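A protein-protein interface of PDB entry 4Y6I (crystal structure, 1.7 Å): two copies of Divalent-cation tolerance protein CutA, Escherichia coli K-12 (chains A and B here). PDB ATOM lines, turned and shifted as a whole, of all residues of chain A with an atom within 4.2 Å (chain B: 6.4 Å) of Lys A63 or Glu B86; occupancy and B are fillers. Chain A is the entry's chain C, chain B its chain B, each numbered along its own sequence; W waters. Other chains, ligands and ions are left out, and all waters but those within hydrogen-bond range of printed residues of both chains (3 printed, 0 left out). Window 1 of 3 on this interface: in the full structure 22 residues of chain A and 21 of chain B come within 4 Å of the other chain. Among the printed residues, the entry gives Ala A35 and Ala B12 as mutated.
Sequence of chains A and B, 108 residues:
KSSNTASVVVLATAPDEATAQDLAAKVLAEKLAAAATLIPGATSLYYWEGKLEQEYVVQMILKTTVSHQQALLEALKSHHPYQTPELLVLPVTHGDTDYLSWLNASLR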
ATOM      1  N   VAL A   8       7.076   3.469 -30.180  1.00  0.00           N
ATOM      2  CA  VAL A   8       7.421   2.173 -30.759  1.00  0.00           C
ATOM      3  C   VAL A   8       8.515   1.540 -29.929  1.00  0.00           C
ATOM      4  O   VAL A   8       9.202   2.218 -29.152  1.00  0.00           O
ATOM      5  CB  VAL A   8       7.960   2.278 -32.223  1.00  0.00           C
ATOM      6  CG1 VAL A   8       6.883   2.829 -33.178  1.00  0.00           C
ATOM      7  CG2 VAL A   8       9.257   3.100 -32.288  1.00  0.00           C
ATOM      8  N   VAL A   9       8.653   0.231 -30.078  1.00  0.00           N
ATOM      9  CA  VAL A   9       9.851  -0.437 -29.569  1.00  0.00           C
ATOM     10  C   VAL A   9      10.650  -0.968 -30.732  1.00  0.00           C
ATOM     11  O   VAL A   9      10.105  -1.343 -31.776  1.00  0.00           O
ATOM     12  CB  VAL A   9       9.587  -1.542 -28.511  1.00  0.00           C
ATOM     13  CG1 VAL A   9       9.016  -0.912 -27.241  1.00  0.00           C
ATOM     14  CG2 VAL A   9       8.680  -2.648 -29.067  1.00  0.00           C
ATOM     15  N   ALA A  33      16.647   7.579 -28.946  1.00  0.00           N
ATOM     16  CA  ALA A  33      15.871   6.640 -28.141  1.00  0.00           C
ATOM     17  C   ALA A  33      15.835   7.192 -26.724  1.00  0.00           C
ATOM     18  O   ALA A  33      16.740   7.935 -26.314  1.00  0.00           O
ATOM     19  CB  ALA A  33      16.514   5.254 -28.165  1.00  0.00           C
ATOM     20  N   ALA A  34      14.788   6.833 -25.986  1.00  0.00           N
ATOM     21  CA  ALA A  34      14.625   7.249 -24.595  1.00  0.00           C
ATOM     22  C   ALA A  34      15.254   6.262 -23.607  1.00  0.00           C
ATOM     23  O   ALA A  34      15.716   6.647 -22.520  1.00  0.00           O
ATOM     24  CB  ALA A  34      13.143   7.440 -24.279  1.00  0.00           C
ATOM     25  N   ALA A  35      15.247   4.982 -23.968  1.00  0.00           N
ATOM     26  CA  ALA A  35      15.731   3.926 -23.078  1.00  0.00           C
ATOM     27  C   ALA A  35      16.028   2.677 -23.877  1.00  0.00           C
ATOM     28  O   ALA A  35      15.476   2.478 -24.972  1.00  0.00           O
ATOM     29  CB  ALA A  35      14.704   3.629 -21.981  1.00  0.00           C
ATOM     30  N   THR A  37      16.713  -1.631 -23.089  1.00  0.00           N
ATOM     31  CA  THR A  37      16.900  -2.802 -22.247  1.00  0.00           C
ATOM     32  C   THR A  37      17.807  -3.776 -22.989  1.00  0.00           C
ATOM     33  O   THR A  37      17.600  -4.037 -24.172  1.00  0.00           O
ATOM     34  CB  THR A  37      15.557  -3.456 -21.927  1.00  0.00           C
ATOM     35  OG1 THR A  37      14.746  -2.518 -21.209  1.00  0.00           O
ATOM     36  CG2 THR A  37      15.761  -4.714 -21.103  1.00  0.00           C
ATOM     37  N   ILE A  61      15.893  -4.088 -26.453  1.00  0.00           N
ATOM     38  CA  ILE A  61      14.561  -3.516 -26.658  1.00  0.00           C
ATOM     39  C   ILE A  61      14.678  -2.013 -26.399  1.00  0.00           C
ATOM     40  O   ILE A  61      14.803  -1.572 -25.243  1.00  0.00           O
ATOM     41  CB  ILE A  61      13.525  -4.127 -25.704  1.00  0.00           C
ATOM     42  CG1 ILE A  61      13.510  -5.658 -25.831  1.00  0.00           C
ATOM     43  CG2 ILE A  61      12.131  -3.558 -25.990  1.00  0.00           C
ATOM     44  CD1 ILE A  61      12.624  -6.351 -24.788  1.00  0.00           C
ATOM     45  N   LEU A  62      14.654  -1.228 -27.471  1.00  0.00           N
ATOM     46  CA  LEU A  62      14.801   0.218 -27.347  1.00  0.00           C
ATOM     47  C   LEU A  62      13.430   0.876 -27.449  1.00  0.00           C
ATOM     48  O   LEU A  62      12.543   0.358 -28.138  1.00  0.00           O
ATOM     49  CB  LEU A  62      15.734   0.764 -28.440  1.00  0.00           C
ATOM     50  CG  LEU A  62      17.159   0.182 -28.428  1.00  0.00           C
ATOM     51  CD1 LEU A  62      17.283  -0.920 -29.479  1.00  0.00           C
ATOM     52  CD2 LEU A  62      18.185   1.274 -28.700  1.00  0.00           C
ATOM     53  N   LYS A  63      13.248   1.995 -26.752  1.00  0.00           N
ATOM     54  CA  LYS A  63      11.985   2.732 -26.789  1.00  0.00           C
ATOM     55  C   LYS A  63      12.216   4.076 -27.446  1.00  0.00           C
ATOM     56  O   LYS A  63      13.144   4.802 -27.085  1.00  0.00           O
ATOM     57  CB  LYS A  63      11.440   2.965 -25.375  1.00  0.00           C
ATOM     58  CG  LYS A  63      10.618   1.806 -24.795  1.00  0.00           C
ATOM     59  CD  LYS A  63      11.430   0.545 -24.519  1.00  0.00           C
ATOM     60  CE  LYS A  63      12.560   0.787 -23.532  1.00  0.00           C
ATOM     61  NZ  LYS A  63      13.070  -0.505 -22.976  1.00  0.00           N
ATOM     62  N   THR A  64      11.359   4.411 -28.407  1.00  0.00           N
ATOM     63  CA  THR A  64      11.430   5.726 -29.037  1.00  0.00           C
ATOM     64  C   THR A  64      10.055   6.131 -29.549  1.00  0.00           C
ATOM     65  O   THR A  64       9.079   5.433 -29.301  1.00  0.00           O
ATOM     66  CB  THR A  64      12.536   5.781 -30.136  1.00  0.00           C
ATOM     67  OG1 THR A  64      12.784   7.147 -30.475  1.00  0.00           O
ATOM     68  CG2 THR A  64      12.139   4.996 -31.397  1.00  0.00           C
ATOM     69  N   TYR A  99       5.041   7.457 -18.215  1.00  0.00           N
ATOM     70  CA  TYR A  99       6.173   6.903 -18.944  1.00  0.00           C
ATOM     71  C   TYR A  99       6.197   7.448 -20.373  1.00  0.00           C
ATOM     72  O   TYR A  99       7.251   7.898 -20.840  1.00  0.00           O
ATOM     73  CB  TYR A  99       6.189   5.363 -18.940  1.00  0.00           C
ATOM     74  CG  TYR A  99       7.428   4.840 -19.625  1.00  0.00           C
ATOM     75  CD1 TYR A  99       8.638   4.738 -18.937  1.00  0.00           C
ATOM     76  CD2 TYR A  99       7.399   4.476 -20.975  1.00  0.00           C
ATOM     77  CE1 TYR A  99       9.788   4.288 -19.578  1.00  0.00           C
ATOM     78  CE2 TYR A  99       8.537   4.023 -21.615  1.00  0.00           C
ATOM     79  CZ  TYR A  99       9.729   3.934 -20.909  1.00  0.00           C
ATOM     80  OH  TYR A  99      10.846   3.488 -21.567  1.00  0.00           O
ATOM     81  N   LEU A 103       9.000   9.641 -22.130  1.00  0.00           N
ATOM     82  CA  LEU A 103       9.608   9.134 -23.353  1.00  0.00           C
ATOM     83  C   LEU A 103       9.657  10.242 -24.419  1.00  0.00           C
ATOM     84  O   LEU A 103      10.710  10.480 -25.028  1.00  0.00           O
ATOM     85  CB  LEU A 103       8.818   7.910 -23.846  1.00  0.00           C
ATOM     86  CG  LEU A 103       9.328   6.932 -24.905  1.00  0.00           C
ATOM     87  CD1 LEU A 103       8.367   5.750 -24.969  1.00  0.00           C
ATOM     88  CD2 LEU A 103       9.460   7.567 -26.275  1.00  0.00           C
ATOM     89  N   LEU B  11       4.661  -5.229 -22.218  1.00  0.00           N
ATOM     90  CA  LEU B  11       6.053  -5.270 -21.779  1.00  0.00           C
ATOM     91  C   LEU B  11       6.181  -4.368 -20.562  1.00  0.00           C
ATOM     92  O   LEU B  11       5.793  -3.188 -20.598  1.00  0.00           O
ATOM     93  CB  LEU B  11       6.998  -4.799 -22.889  1.00  0.00           C
ATOM     94  CG  LEU B  11       7.046  -5.621 -24.173  1.00  0.00           C
ATOM     95  CD1 LEU B  11       8.049  -4.975 -25.151  1.00  0.00           C
ATOM     96  CD2 LEU B  11       7.406  -7.072 -23.905  1.00  0.00           C
ATOM     97  N   ALA B  12       6.686  -4.930 -19.475  1.00  0.00           N
ATOM     98  CA  ALA B  12       6.893  -4.174 -18.240  1.00  0.00           C
ATOM     99  C   ALA B  12       8.264  -4.501 -17.696  1.00  0.00           C
ATOM    100  O   ALA B  12       8.705  -5.642 -17.779  1.00  0.00           O
ATOM    101  CB  ALA B  12       5.826  -4.517 -17.207  1.00  0.00           C
ATOM    102  N   THR B  13       8.953  -3.512 -17.140  1.00  0.00           N
ATOM    103  CA  THR B  13      10.188  -3.826 -16.416  1.00  0.00           C
ATOM    104  C   THR B  13       9.994  -3.618 -14.921  1.00  0.00           C
ATOM    105  O   THR B  13       9.233  -2.736 -14.488  1.00  0.00           O
ATOM    106  CB  THR B  13      11.403  -3.038 -16.906  1.00  0.00           C
ATOM    107  OG1 THR B  13      11.208  -1.650 -16.647  1.00  0.00           O
ATOM    108  CG2 THR B  13      11.616  -3.246 -18.399  1.00  0.00           C
ATOM    109  N   ALA B  14      10.686  -4.454 -14.156  1.00  0.00           N
ATOM    110  CA  ALA B  14      10.694  -4.394 -12.701  1.00  0.00           C
ATOM    111  C   ALA B  14      12.147  -4.265 -12.253  1.00  0.00           C
ATOM    112  O   ALA B  14      13.050  -4.733 -12.946  1.00  0.00           O
ATOM    113  CB  ALA B  14      10.071  -5.662 -12.130  1.00  0.00           C
ATOM    114  N   SER B  44      18.862  -1.916 -17.958  1.00  0.00           N
ATOM    115  CA  SER B  44      18.193  -0.782 -18.595  1.00  0.00           C
ATOM    116  C   SER B  44      19.096   0.435 -18.560  1.00  0.00           C
ATOM    117  O   SER B  44      19.644   0.773 -17.503  1.00  0.00           O
ATOM    118  CB  SER B  44      16.861  -0.463 -17.921  1.00  0.00           C
ATOM    119  OG  SER B  44      16.282   0.737 -18.437  1.00  0.00           O
ATOM    120  N   GLN B  59      12.850  -8.125 -17.294  1.00  0.00           N
ATOM    121  CA  GLN B  59      11.891  -7.881 -18.365  1.00  0.00           C
ATOM    122  C   GLN B  59      10.683  -8.782 -18.160  1.00  0.00           C
ATOM    123  O   GLN B  59      10.832 -10.000 -18.050  1.00  0.00           O
ATOM    124  CB  GLN B  59      12.505  -8.144 -19.748  1.00  0.00           C
ATOM    125  CG  GLN B  59      11.505  -7.864 -20.913  1.00  0.00           C
ATOM    126  CD  GLN B  59      11.159  -6.384 -21.025  1.00  0.00           C
ATOM    127  OE1 GLN B  59      12.030  -5.559 -21.266  1.00  0.00           O
ATOM    128  NE2 GLN B  59       9.877  -6.040 -20.843  1.00  0.00           N
ATOM    129  N   HIS B  80       3.873  -1.025  -8.634  1.00  0.00           N
ATOM    130  CA  HIS B  80       5.271  -0.739  -8.971  1.00  0.00           C
ATOM    131  C   HIS B  80       5.864   0.287  -8.002  1.00  0.00           C
ATOM    132  O   HIS B  80       5.251   1.323  -7.743  1.00  0.00           O
ATOM    133  CB  HIS B  80       5.369  -0.211 -10.404  1.00  0.00           C
ATOM    134  CG  HIS B  80       6.698  -0.440 -11.054  1.00  0.00           C
ATOM    135  ND1 HIS B  80       7.830   0.268 -10.709  1.00  0.00           N
ATOM    136  CD2 HIS B  80       7.073  -1.294 -12.037  1.00  0.00           C
ATOM    137  CE1 HIS B  80       8.844  -0.135 -11.457  1.00  0.00           C
ATOM    138  NE2 HIS B  80       8.410  -1.082 -12.271  1.00  0.00           N
ATOM    139  N   THR B  84       7.658   6.293 -12.548  1.00  0.00           N
ATOM    140  CA  THR B  84       7.546   6.368 -14.006  1.00  0.00           C
ATOM    141  C   THR B  84       7.850   4.985 -14.604  1.00  0.00           C
ATOM    142  O   THR B  84       8.865   4.811 -15.273  1.00  0.00           O
ATOM    143  CB  THR B  84       8.485   7.463 -14.575  1.00  0.00           C
ATOM    144  OG1 THR B  84       8.234   8.706 -13.896  1.00  0.00           O
ATOM    145  CG2 THR B  84       8.259   7.668 -16.069  1.00  0.00           C
ATOM    146  N   PRO B  85       6.967   3.996 -14.358  1.00  0.00           N
ATOM    147  CA  PRO B  85       7.302   2.622 -14.714  1.00  0.00           C
ATOM    148  C   PRO B  85       7.169   2.377 -16.212  1.00  0.00           C
ATOM    149  O   PRO B  85       6.233   2.884 -16.844  1.00  0.00           O
ATOM    150  CB  PRO B  85       6.252   1.802 -13.955  1.00  0.00           C
ATOM    151  CG  PRO B  85       5.070   2.687 -13.907  1.00  0.00           C
ATOM    152  CD  PRO B  85       5.602   4.095 -13.806  1.00  0.00           C
ATOM    153  N   GLU B  86       8.104   1.603 -16.753  1.00  0.00           N
ATOM    154  CA  GLU B  86       8.087   1.246 -18.169  1.00  0.00           C
ATOM    155  C   GLU B  86       7.059   0.149 -18.420  1.00  0.00           C
ATOM    156  O   GLU B  86       7.344  -1.043 -18.220  1.00  0.00           O
ATOM    157  CB  GLU B  86       9.474   0.798 -18.621  1.00  0.00           C
ATOM    158  CG  GLU B  86       9.532   0.507 -20.114  1.00  0.00           C
ATOM    159  CD  GLU B  86      10.804  -0.185 -20.534  1.00  0.00           C
ATOM    160  OE1 GLU B  86      11.879   0.115 -19.962  1.00  0.00           O
ATOM    161  OE2 GLU B  86      10.717  -1.033 -21.450  1.00  0.00           O
ATOM    162  N   LEU B  87       5.874   0.571 -18.853  1.00  0.00           N
ATOM    163  CA  LEU B  87       4.733  -0.309 -19.097  1.00  0.00           C
ATOM    164  C   LEU B  87       4.173   0.022 -20.470  1.00  0.00           C
ATOM    165  O   LEU B  87       3.706   1.147 -20.699  1.00  0.00           O
ATOM    166  CB  LEU B  87       3.641  -0.078 -18.050  1.00  0.00           C
ATOM    167  CG  LEU B  87       4.021  -0.013 -16.576  1.00  0.00           C
ATOM    168  CD1 LEU B  87       2.767   0.328 -15.767  1.00  0.00           C
ATOM    169  CD2 LEU B  87       4.654  -1.332 -16.116  1.00  0.00           C
ATOM    170  N   LEU B  88       4.243  -0.950 -21.384  1.00  0.00           N
ATOM    171  CA  LEU B  88       3.929  -0.725 -22.812  1.00  0.00           C
ATOM    172  C   LEU B  88       3.035  -1.818 -23.357  1.00  0.00           C
ATOM    173  O   LEU B  88       3.245  -2.986 -23.054  1.00  0.00           O
ATOM    174  CB  LEU B  88       5.227  -0.715 -23.636  1.00  0.00           C
ATOM    175  CG  LEU B  88       6.285   0.278 -23.161  1.00  0.00           C
ATOM    176  CD1 LEU B  88       7.639  -0.028 -23.818  1.00  0.00           C
ATOM    177  CD2 LEU B  88       5.840   1.709 -23.413  1.00  0.00           C
HETATM  178  O   HOH W   1      12.202  -3.050 -21.959  1.00  0.00           O
HETATM  179  O   HOH W   2      14.872   0.151 -20.812  1.00  0.00           O
HETATM  180  O   HOH W   3      12.738   2.834 -19.514  1.00  0.00           O
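OE2 of Glu B86 lies within salt-bridge range of NZ of Lys A63 (2.9 Å).
O of Ala B12 lies within hydrogen-bond range of NE2 of Gln B59 (3.3 Å).
N of Leu B11 is in hydrogen-bond range of O of Leu B88, at 2.8 Å.
O of Ala A35 lies within hydrogen-bond range of N of Lys A63, 2.9 Å away.
The side-chain hydroxyl (OG1) of Thr A37 lies within hydrogen-bond range of the side-chain amino group (NZ) of Lys A63 (3.2 Å).
O of Ile A61 lies within hydrogen-bond range of NZ of Lys A63 (3.0 Å).
The backbone carbonyl oxygen of Glu B86 lies within hydrogen-bond range of the backbone NH of Thr B13.
Among the printed residues, pairs that only touch across the chains: Tyr A99 with Pro B85, Tyr A99 with Glu B86, Lys A63 with Leu B88, Tyr A99 with Thr B84, Ile A61 with Gln B59, Val A9 with Leu B88, Thr A37 with Gln B59 and Tyr A99 with Leu B88.
Of chain B, only Glu B86 and Leu B88 come within 4 Å of Lys A63.
Of chain A, only Lys A63 (2.9 Å) and Tyr A99 (3.5 Å) come within 4 Å of Glu B86.
Printed residues of chain A within 4 Å of Pro B85: Tyr A99 (3.2 Å).
Of the printed residues of chain A, Thr B84 touches Tyr A99.
Printed residues of chain A within 4 Å of Gln B59: Thr A37 and Ile A61.
Printed residues of chain B within 4 Å of Tyr A99: Thr B84 (3.6 Å), Pro B85 (3.2 Å), Glu B86 (3.5 Å) and Leu B88 (3.98 Å).
The nearest printed residue of chain A that does not touch Thr B84 is Leu A103 (6.4 Å).
Printed residues of chain A that touch a printed residue of chain B: Val A9, Thr A37, Ile A61, Lys A63 and Tyr A99.
Printed residues of chain B that touch a printed residue of chain A: Gln B59, Thr B84, Pro B85, Glu B86 and Leu B88.
Among the printed residues, 9 pairs touch across the chains.
No position is printed for both chains.
Of the 9 pairs that touch across the chains among the printed residues, none has its exchanged pair printed and touching as well.
Water W1 lies within hydrogen-bond range of the side-chain carboxylate (OE2) of Glu B86, the side-chain amide oxygen (OE1) of Gln B59, the side-chain hydroxyl (OG1) of Thr A37 and the side-chain amino group (NZ) of Lys A63.
Water W2 lies within hydrogen-bond range of OG1 of Thr A37 (2.7 Å), OG of Ser B44 (2.8 Å), NZ of Lys A63 (2.9 Å) and OE1 of Glu B86 (3.1 Å).
Water W3 lies within hydrogen-bond range of OH of Tyr A99 (2.9 Å) and OE1 of Glu B86 (2.9 Å).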
